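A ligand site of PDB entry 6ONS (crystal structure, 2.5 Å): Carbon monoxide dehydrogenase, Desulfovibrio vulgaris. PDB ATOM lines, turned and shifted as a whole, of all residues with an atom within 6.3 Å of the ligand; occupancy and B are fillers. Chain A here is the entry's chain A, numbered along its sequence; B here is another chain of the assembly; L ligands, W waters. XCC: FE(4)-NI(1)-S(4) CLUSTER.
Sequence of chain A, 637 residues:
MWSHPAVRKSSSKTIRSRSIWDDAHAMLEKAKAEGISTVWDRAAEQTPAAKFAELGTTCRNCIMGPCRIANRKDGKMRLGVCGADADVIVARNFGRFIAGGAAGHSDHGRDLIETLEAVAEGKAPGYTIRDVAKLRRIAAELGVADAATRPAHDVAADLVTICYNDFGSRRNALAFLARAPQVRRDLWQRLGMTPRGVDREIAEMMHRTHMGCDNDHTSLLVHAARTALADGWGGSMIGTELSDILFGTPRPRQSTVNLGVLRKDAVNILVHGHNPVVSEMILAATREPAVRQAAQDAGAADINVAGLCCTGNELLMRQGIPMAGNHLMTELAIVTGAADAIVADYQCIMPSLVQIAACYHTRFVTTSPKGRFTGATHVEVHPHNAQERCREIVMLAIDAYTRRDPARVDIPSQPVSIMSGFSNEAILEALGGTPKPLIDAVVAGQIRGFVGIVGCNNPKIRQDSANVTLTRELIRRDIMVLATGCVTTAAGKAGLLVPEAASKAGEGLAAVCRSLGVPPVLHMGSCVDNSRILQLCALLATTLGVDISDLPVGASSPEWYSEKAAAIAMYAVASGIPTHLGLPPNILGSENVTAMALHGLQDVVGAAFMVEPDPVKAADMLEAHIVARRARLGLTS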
ATOM      1  N   HIS A 272     -16.349  31.654  -1.327  1.00  0.00           N
ATOM      2  CA  HIS A 272     -17.413  30.717  -1.617  1.00  0.00           C
ATOM      3  C   HIS A 272     -16.849  29.550  -2.410  1.00  0.00           C
ATOM      4  O   HIS A 272     -15.893  29.710  -3.181  1.00  0.00           O
ATOM      5  CB  HIS A 272     -18.555  31.395  -2.385  1.00  0.00           C
ATOM      6  CG  HIS A 272     -19.853  30.644  -2.359  1.00  0.00           C
ATOM      7  ND1 HIS A 272     -20.028  29.484  -1.643  1.00  0.00           N
ATOM      8  CD2 HIS A 272     -21.044  30.907  -2.953  1.00  0.00           C
ATOM      9  CE1 HIS A 272     -21.269  29.054  -1.806  1.00  0.00           C
ATOM     10  NE2 HIS A 272     -21.900  29.899  -2.599  1.00  0.00           N
ATOM     11  N   GLY A 273     -17.434  28.365  -2.215  1.00  0.00           N
ATOM     12  CA  GLY A 273     -17.016  27.177  -2.946  1.00  0.00           C
ATOM     13  C   GLY A 273     -16.509  26.102  -1.997  1.00  0.00           C
ATOM     14  O   GLY A 273     -17.049  25.909  -0.909  1.00  0.00           O
ATOM     15  N   HIS A 274     -15.462  25.389  -2.441  1.00  0.00           N
ATOM     16  CA  HIS A 274     -15.022  24.195  -1.748  1.00  0.00           C
ATOM     17  C   HIS A 274     -13.510  24.086  -1.603  1.00  0.00           C
ATOM     18  O   HIS A 274     -13.012  23.686  -0.540  1.00  0.00           O
ATOM     19  CB  HIS A 274     -15.552  22.946  -2.467  1.00  0.00           C
ATOM     20  CG  HIS A 274     -16.982  22.640  -2.181  1.00  0.00           C
ATOM     21  ND1 HIS A 274     -18.022  23.460  -2.578  1.00  0.00           N
ATOM     22  CD2 HIS A 274     -17.554  21.611  -1.513  1.00  0.00           C
ATOM     23  CE1 HIS A 274     -19.166  22.940  -2.170  1.00  0.00           C
ATOM     24  NE2 HIS A 274     -18.910  21.816  -1.524  1.00  0.00           N
ATOM     25  N   CYS A 309     -20.105  28.156   2.965  1.00  0.00           N
ATOM     26  CA  CYS A 309     -20.240  26.746   2.553  1.00  0.00           C
ATOM     27  C   CYS A 309     -18.966  25.994   2.950  1.00  0.00           C
ATOM     28  O   CYS A 309     -18.427  26.221   4.040  1.00  0.00           O
ATOM     29  CB  CYS A 309     -20.596  26.681   1.079  1.00  0.00           C
ATOM     30  SG  CYS A 309     -22.315  27.124   0.737  1.00  0.00           S
ATOM     31  N   CYS A 310     -18.460  25.104   2.094  1.00  0.00           N
ATOM     32  CA  CYS A 310     -17.393  24.193   2.509  1.00  0.00           C
ATOM     33  C   CYS A 310     -16.030  24.861   2.557  1.00  0.00           C
ATOM     34  O   CYS A 310     -15.214  24.533   3.418  1.00  0.00           O
ATOM     35  CB  CYS A 310     -17.355  22.979   1.574  1.00  0.00           C
ATOM     36  SG  CYS A 310     -18.535  21.703   2.009  1.00  0.00           S
ATOM     37  N   ASN A 326     -24.370  29.334   5.286  1.00  0.00           N
ATOM     38  CA  ASN A 326     -24.347  28.088   4.528  1.00  0.00           C
ATOM     39  C   ASN A 326     -25.053  28.293   3.190  1.00  0.00           C
ATOM     40  O   ASN A 326     -25.091  29.427   2.670  1.00  0.00           O
ATOM     41  CB  ASN A 326     -24.939  26.976   5.391  1.00  0.00           C
ATOM     42  CG  ASN A 326     -26.317  27.309   5.918  1.00  0.00           C
ATOM     43  OD1 ASN A 326     -26.908  28.317   5.551  1.00  0.00           O
ATOM     44  ND2 ASN A 326     -26.835  26.456   6.803  1.00  0.00           N
ATOM     45  N   HIS A 327     -25.630  27.217   2.645  1.00  0.00           N
ATOM     46  CA  HIS A 327     -26.170  27.208   1.284  1.00  0.00           C
ATOM     47  C   HIS A 327     -27.185  28.309   1.036  1.00  0.00           C
ATOM     48  O   HIS A 327     -26.917  29.243   0.278  1.00  0.00           O
ATOM     49  CB  HIS A 327     -26.801  25.846   0.991  1.00  0.00           C
ATOM     50  CG  HIS A 327     -27.393  25.747  -0.381  1.00  0.00           C
ATOM     51  ND1 HIS A 327     -28.554  25.059  -0.649  1.00  0.00           N
ATOM     52  CD2 HIS A 327     -26.975  26.246  -1.568  1.00  0.00           C
ATOM     53  CE1 HIS A 327     -28.831  25.135  -1.935  1.00  0.00           C
ATOM     54  NE2 HIS A 327     -27.890  25.851  -2.518  1.00  0.00           N
ATOM     55  N   GLN A 347     -18.710  24.421  -7.392  1.00  0.00           N
ATOM     56  CA  GLN A 347     -19.694  23.649  -6.626  1.00  0.00           C
ATOM     57  C   GLN A 347     -20.563  24.509  -5.722  1.00  0.00           C
ATOM     58  O   GLN A 347     -20.060  25.249  -4.871  1.00  0.00           O
ATOM     59  CB  GLN A 347     -19.004  22.550  -5.809  1.00  0.00           C
ATOM     60  CG  GLN A 347     -18.353  21.468  -6.639  1.00  0.00           C
ATOM     61  CD  GLN A 347     -17.664  20.419  -5.790  1.00  0.00           C
ATOM     62  OE1 GLN A 347     -17.978  20.256  -4.604  1.00  0.00           O
ATOM     63  NE2 GLN A 347     -16.730  19.693  -6.377  1.00  0.00           N
ATOM     64  N   CYS A 348     -21.884  24.411  -5.916  1.00  0.00           N
ATOM     65  CA  CYS A 348     -22.899  25.001  -5.053  1.00  0.00           C
ATOM     66  C   CYS A 348     -22.900  26.529  -5.064  1.00  0.00           C
ATOM     67  O   CYS A 348     -23.475  27.154  -4.169  1.00  0.00           O
ATOM     68  CB  CYS A 348     -22.776  24.495  -3.614  1.00  0.00           C
ATOM     69  SG  CYS A 348     -22.868  22.714  -3.516  1.00  0.00           S
ATOM     70  N   VAL A 454     -24.875  15.412   8.403  1.00  0.00           N
ATOM     71  CA  VAL A 454     -24.221  15.996   7.247  1.00  0.00           C
ATOM     72  C   VAL A 454     -25.295  16.446   6.273  1.00  0.00           C
ATOM     73  O   VAL A 454     -26.437  16.005   6.333  1.00  0.00           O
ATOM     74  CB  VAL A 454     -23.259  14.980   6.587  1.00  0.00           C
ATOM     75  CG1 VAL A 454     -24.034  13.784   6.065  1.00  0.00           C
ATOM     76  CG2 VAL A 454     -22.439  15.623   5.474  1.00  0.00           C
ATOM     77  N   GLY A 455     -24.926  17.366   5.395  1.00  0.00           N
ATOM     78  CA  GLY A 455     -25.801  17.695   4.296  1.00  0.00           C
ATOM     79  C   GLY A 455     -26.030  19.175   4.166  1.00  0.00           C
ATOM     80  O   GLY A 455     -25.335  20.001   4.771  1.00  0.00           O
ATOM     81  N   CYS A 456     -27.033  19.522   3.366  1.00  0.00           N
ATOM     82  CA  CYS A 456     -27.249  20.845   2.826  1.00  0.00           C
ATOM     83  C   CYS A 456     -28.466  21.501   3.479  1.00  0.00           C
ATOM     84  O   CYS A 456     -28.993  21.042   4.494  1.00  0.00           O
ATOM     85  CB  CYS A 456     -27.453  20.756   1.317  1.00  0.00           C
ATOM     86  SG  CYS A 456     -26.630  19.349   0.550  1.00  0.00           S
ATOM     87  N   ASN A 457     -28.897  22.602   2.873  1.00  0.00           N
ATOM     88  CA  ASN A 457     -30.245  23.112   3.029  1.00  0.00           C
ATOM     89  C   ASN A 457     -31.058  22.758   1.781  1.00  0.00           C
ATOM     90  O   ASN A 457     -30.531  22.275   0.787  1.00  0.00           O
ATOM     91  CB  ASN A 457     -30.226  24.639   3.232  1.00  0.00           C
ATOM     92  CG  ASN A 457     -29.380  25.053   4.407  1.00  0.00           C
ATOM     93  OD1 ASN A 457     -28.562  25.967   4.305  1.00  0.00           O
ATOM     94  ND2 ASN A 457     -29.557  24.386   5.552  1.00  0.00           N
ATOM     95  N   THR A 484     -20.630  17.958   9.800  1.00  0.00           N
ATOM     96  CA  THR A 484     -19.822  18.379   8.664  1.00  0.00           C
ATOM     97  C   THR A 484     -20.696  19.124   7.667  1.00  0.00           C
ATOM     98  O   THR A 484     -21.929  19.066   7.736  1.00  0.00           O
ATOM     99  CB  THR A 484     -19.149  17.179   7.951  1.00  0.00           C
ATOM    100  OG1 THR A 484     -20.156  16.235   7.577  1.00  0.00           O
ATOM    101  CG2 THR A 484     -18.123  16.508   8.858  1.00  0.00           C
ATOM    102  N   GLY A 485     -20.044  19.834   6.750  1.00  0.00           N
ATOM    103  CA  GLY A 485     -20.786  20.509   5.703  1.00  0.00           C
ATOM    104  C   GLY A 485     -21.575  21.701   6.221  1.00  0.00           C
ATOM    105  O   GLY A 485     -21.206  22.361   7.184  1.00  0.00           O
ATOM    106  N   CYS A 486     -22.705  21.966   5.543  1.00  0.00           N
ATOM    107  CA  CYS A 486     -23.528  23.118   5.883  1.00  0.00           C
ATOM    108  C   CYS A 486     -24.298  22.963   7.189  1.00  0.00           C
ATOM    109  O   CYS A 486     -24.847  23.945   7.682  1.00  0.00           O
ATOM    110  CB  CYS A 486     -24.510  23.416   4.740  1.00  0.00           C
ATOM    111  SG  CYS A 486     -23.773  24.326   3.369  1.00  0.00           S
ATOM    112  N   VAL A 487     -24.335  21.752   7.746  1.00  0.00           N
ATOM    113  CA  VAL A 487     -24.966  21.573   9.056  1.00  0.00           C
ATOM    114  C   VAL A 487     -24.152  22.239  10.150  1.00  0.00           C
ATOM    115  O   VAL A 487     -24.678  22.517  11.234  1.00  0.00           O
ATOM    116  CB  VAL A 487     -25.162  20.071   9.339  1.00  0.00           C
ATOM    117  CG1 VAL A 487     -26.096  19.873  10.523  1.00  0.00           C
ATOM    118  CG2 VAL A 487     -25.701  19.370   8.113  1.00  0.00           C
ATOM    119  N   SER A 526     -15.603  20.032   6.323  1.00  0.00           N
ATOM    120  CA  SER A 526     -16.443  20.224   5.160  1.00  0.00           C
ATOM    121  C   SER A 526     -17.012  18.882   4.694  1.00  0.00           C
ATOM    122  O   SER A 526     -16.899  17.862   5.369  1.00  0.00           O
ATOM    123  CB  SER A 526     -15.641  20.923   4.058  1.00  0.00           C
ATOM    124  OG  SER A 526     -14.478  20.183   3.727  1.00  0.00           O
ATOM    125  N   CYS A 527     -17.629  18.878   3.505  1.00  0.00           N
ATOM    126  CA  CYS A 527     -18.234  17.662   2.991  1.00  0.00           C
ATOM    127  C   CYS A 527     -17.200  16.588   2.709  1.00  0.00           C
ATOM    128  O   CYS A 527     -17.411  15.408   3.007  1.00  0.00           O
ATOM    129  CB  CYS A 527     -19.040  17.956   1.737  1.00  0.00           C
ATOM    130  SG  CYS A 527     -20.562  18.858   2.025  1.00  0.00           S
ATOM    131  N   TYR A 561     -29.726  18.266  -0.812  1.00  0.00           N
ATOM    132  CA  TYR A 561     -30.195  18.680  -2.134  1.00  0.00           C
ATOM    133  C   TYR A 561     -29.333  18.192  -3.281  1.00  0.00           C
ATOM    134  O   TYR A 561     -29.879  17.935  -4.364  1.00  0.00           O
ATOM    135  CB  TYR A 561     -30.290  20.216  -2.215  1.00  0.00           C
ATOM    136  CG  TYR A 561     -29.095  20.878  -2.883  1.00  0.00           C
ATOM    137  CD1 TYR A 561     -29.105  21.164  -4.249  1.00  0.00           C
ATOM    138  CD2 TYR A 561     -27.956  21.206  -2.163  1.00  0.00           C
ATOM    139  CE1 TYR A 561     -28.016  21.755  -4.862  1.00  0.00           C
ATOM    140  CE2 TYR A 561     -26.869  21.796  -2.765  1.00  0.00           C
ATOM    141  CZ  TYR A 561     -26.905  22.066  -4.115  1.00  0.00           C
ATOM    142  OH  TYR A 561     -25.817  22.656  -4.718  1.00  0.00           O
ATOM    143  N   SER A 562     -28.024  18.027  -3.112  1.00  0.00           N
ATOM    144  CA  SER A 562     -27.125  17.858  -4.239  1.00  0.00           C
ATOM    145  C   SER A 562     -26.901  16.385  -4.572  1.00  0.00           C
ATOM    146  O   SER A 562     -27.123  15.496  -3.737  1.00  0.00           O
ATOM    147  CB  SER A 562     -25.777  18.529  -3.931  1.00  0.00           C
ATOM    148  OG  SER A 562     -25.180  17.983  -2.773  1.00  0.00           O
ATOM    149  N   LYS A 564     -24.128  15.408  -4.603  1.00  0.00           N
ATOM    150  CA  LYS A 564     -22.962  15.143  -3.780  1.00  0.00           C
ATOM    151  C   LYS A 564     -23.355  14.513  -2.446  1.00  0.00           C
ATOM    152  O   LYS A 564     -22.705  13.566  -1.989  1.00  0.00           O
ATOM    153  CB  LYS A 564     -22.190  16.446  -3.575  1.00  0.00           C
ATOM    154  CG  LYS A 564     -20.712  16.284  -3.437  1.00  0.00           C
ATOM    155  CD  LYS A 564     -20.009  17.571  -3.844  1.00  0.00           C
ATOM    156  CE  LYS A 564     -20.870  18.798  -3.555  1.00  0.00           C
ATOM    157  NZ  LYS A 564     -20.130  20.077  -3.717  1.00  0.00           N
ATOM    158  N   ALA A 565     -24.418  15.029  -1.814  1.00  0.00           N
ATOM    159  CA  ALA A 565     -24.899  14.428  -0.579  1.00  0.00           C
ATOM    160  C   ALA A 565     -25.426  13.015  -0.803  1.00  0.00           C
ATOM    161  O   ALA A 565     -25.285  12.148   0.075  1.00  0.00           O
ATOM    162  CB  ALA A 565     -25.982  15.312   0.040  1.00  0.00           C
ATOM    163  N   HIS B 210     -22.616  19.708 -12.431  1.00  0.00           N
ATOM    164  CA  HIS B 210     -23.212  19.757 -11.105  1.00  0.00           C
ATOM    165  C   HIS B 210     -23.729  21.160 -10.818  1.00  0.00           C
ATOM    166  O   HIS B 210     -23.288  22.144 -11.423  1.00  0.00           O
ATOM    167  CB  HIS B 210     -22.193  19.324 -10.045  1.00  0.00           C
ATOM    168  CG  HIS B 210     -22.777  19.150  -8.679  1.00  0.00           C
ATOM    169  ND1 HIS B 210     -22.925  20.198  -7.785  1.00  0.00           N
ATOM    170  CD2 HIS B 210     -23.240  18.046  -8.043  1.00  0.00           C
ATOM    171  CE1 HIS B 210     -23.461  19.744  -6.670  1.00  0.00           C
ATOM    172  NE2 HIS B 210     -23.660  18.440  -6.790  1.00  0.00           N
HETATM  173 FE1  XCC L   1     -23.051  22.064  -1.132  1.00  0.00          FE
HETATM  174 FE2  XCC L   1     -20.241  21.520   0.275  1.00  0.00          FE
HETATM  175 FE3  XCC L   1     -24.504  20.590   0.411  1.00  0.00          FE
HETATM  176 FE4  XCC L   1     -23.306  22.696   1.563  1.00  0.00          FE
HETATM  177  S1  XCC L   1     -23.437  20.597   2.396  1.00  0.00           S
HETATM  178  S2  XCC L   1     -24.937  22.807  -0.076  1.00  0.00           S
HETATM  179  S4  XCC L   1     -23.277  19.785  -1.246  1.00  0.00           S
HETATM  180  S3  XCC L   1     -21.595  23.336   0.238  1.00  0.00           S
HETATM  181  O   HOH W   1     -20.506  19.704  -0.474  1.00  0.00           O
HETATM  182  O   HOH W   2     -21.845  17.393   0.212  1.00  0.00           O
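The side-chain sulfur (SG) of Cys 310 is bound to an iron atom (FE2) of the ligand, 2.4 Å away.
SG of Cys 348 binds FE1 of the ligand.
FE4 of the ligand is bound by SG of Cys 486 (2.5 Å).
An iron atom (FE3) of the ligand is bound by the side-chain sulfur (SG) of Cys 456 (2.5 Å).
The side-chain hydroxyl (OG) of Ser 562 lies close to a sulfur (S4) of the ligand, 3.0 Å away.
NE2 of His 274 is bound to FE2 of the ligand, 2.3 Å away.
The backbone NH (N) of Cys 486 sits close to a sulfur (S1) of the ligand, 3.5 Å away.
A sulfur (S1) of the ligand lies close to the side-chain sulfur (SG) of Cys 527, 3.4 Å away.
The backbone NH (N) of Cys 310 lies within hydrogen-bond range of the backbone carbonyl oxygen (O) of Gly 273 (3.4 Å).
SG of Cys 486 lies close to N of His 327, at 3.5 Å.
SG of Cys 310 lies close to N of Cys 527, at 3.3 Å.
The backbone carbonyl oxygen of Cys 486 lies within hydrogen-bond range of the side-chain amide nitrogen of Asn 326 (3.3 Å).
The side-chain sulfur of Cys 348 sits close to the side-chain hydroxyl of Tyr 561, 3.2 Å away.
The backbone NH (N) of Lys 564 lies close to the side-chain hydroxyl (OG) of Ser 562, 3.3 Å away.
The backbone NH (N) of Tyr 561 sits close to the side-chain sulfur (SG) of Cys 456, 3.6 Å away.
The backbone NH (N) of Cys 486 sits at hydrogen-bond distance from the backbone carbonyl oxygen (O) of Gly 455.
A sulfur (S1) of the ligand sits close to the backbone carbonyl oxygen (O) of Gly 455 (3.1 Å).
Cys 309 touches the ligand.
CB of His 327 touches S2 of the ligand, at 3.7 Å.
Tyr 561 touches the ligand.
CE of Lys 564 touches S4 of the ligand, 3.5 Å away.
Hydrophobic or aromatic side chains within 4 Å of the ligand: His 274, His 327 and Tyr 561.
Of the 24 residues printed, 12 come within 4 Å of the ligand.
The nearest printed residue that does not touch the ligand is Gly 485 (4.2 Å).
Water W1 bridges the side-chain sulfur of Cys 527 (2.6 Å) and the side-chain amino group of Lys 564 (3.3 Å).
Water W2 bridges SG of Cys 527 (2.7 Å) and S4 of the ligand (3.1 Å).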
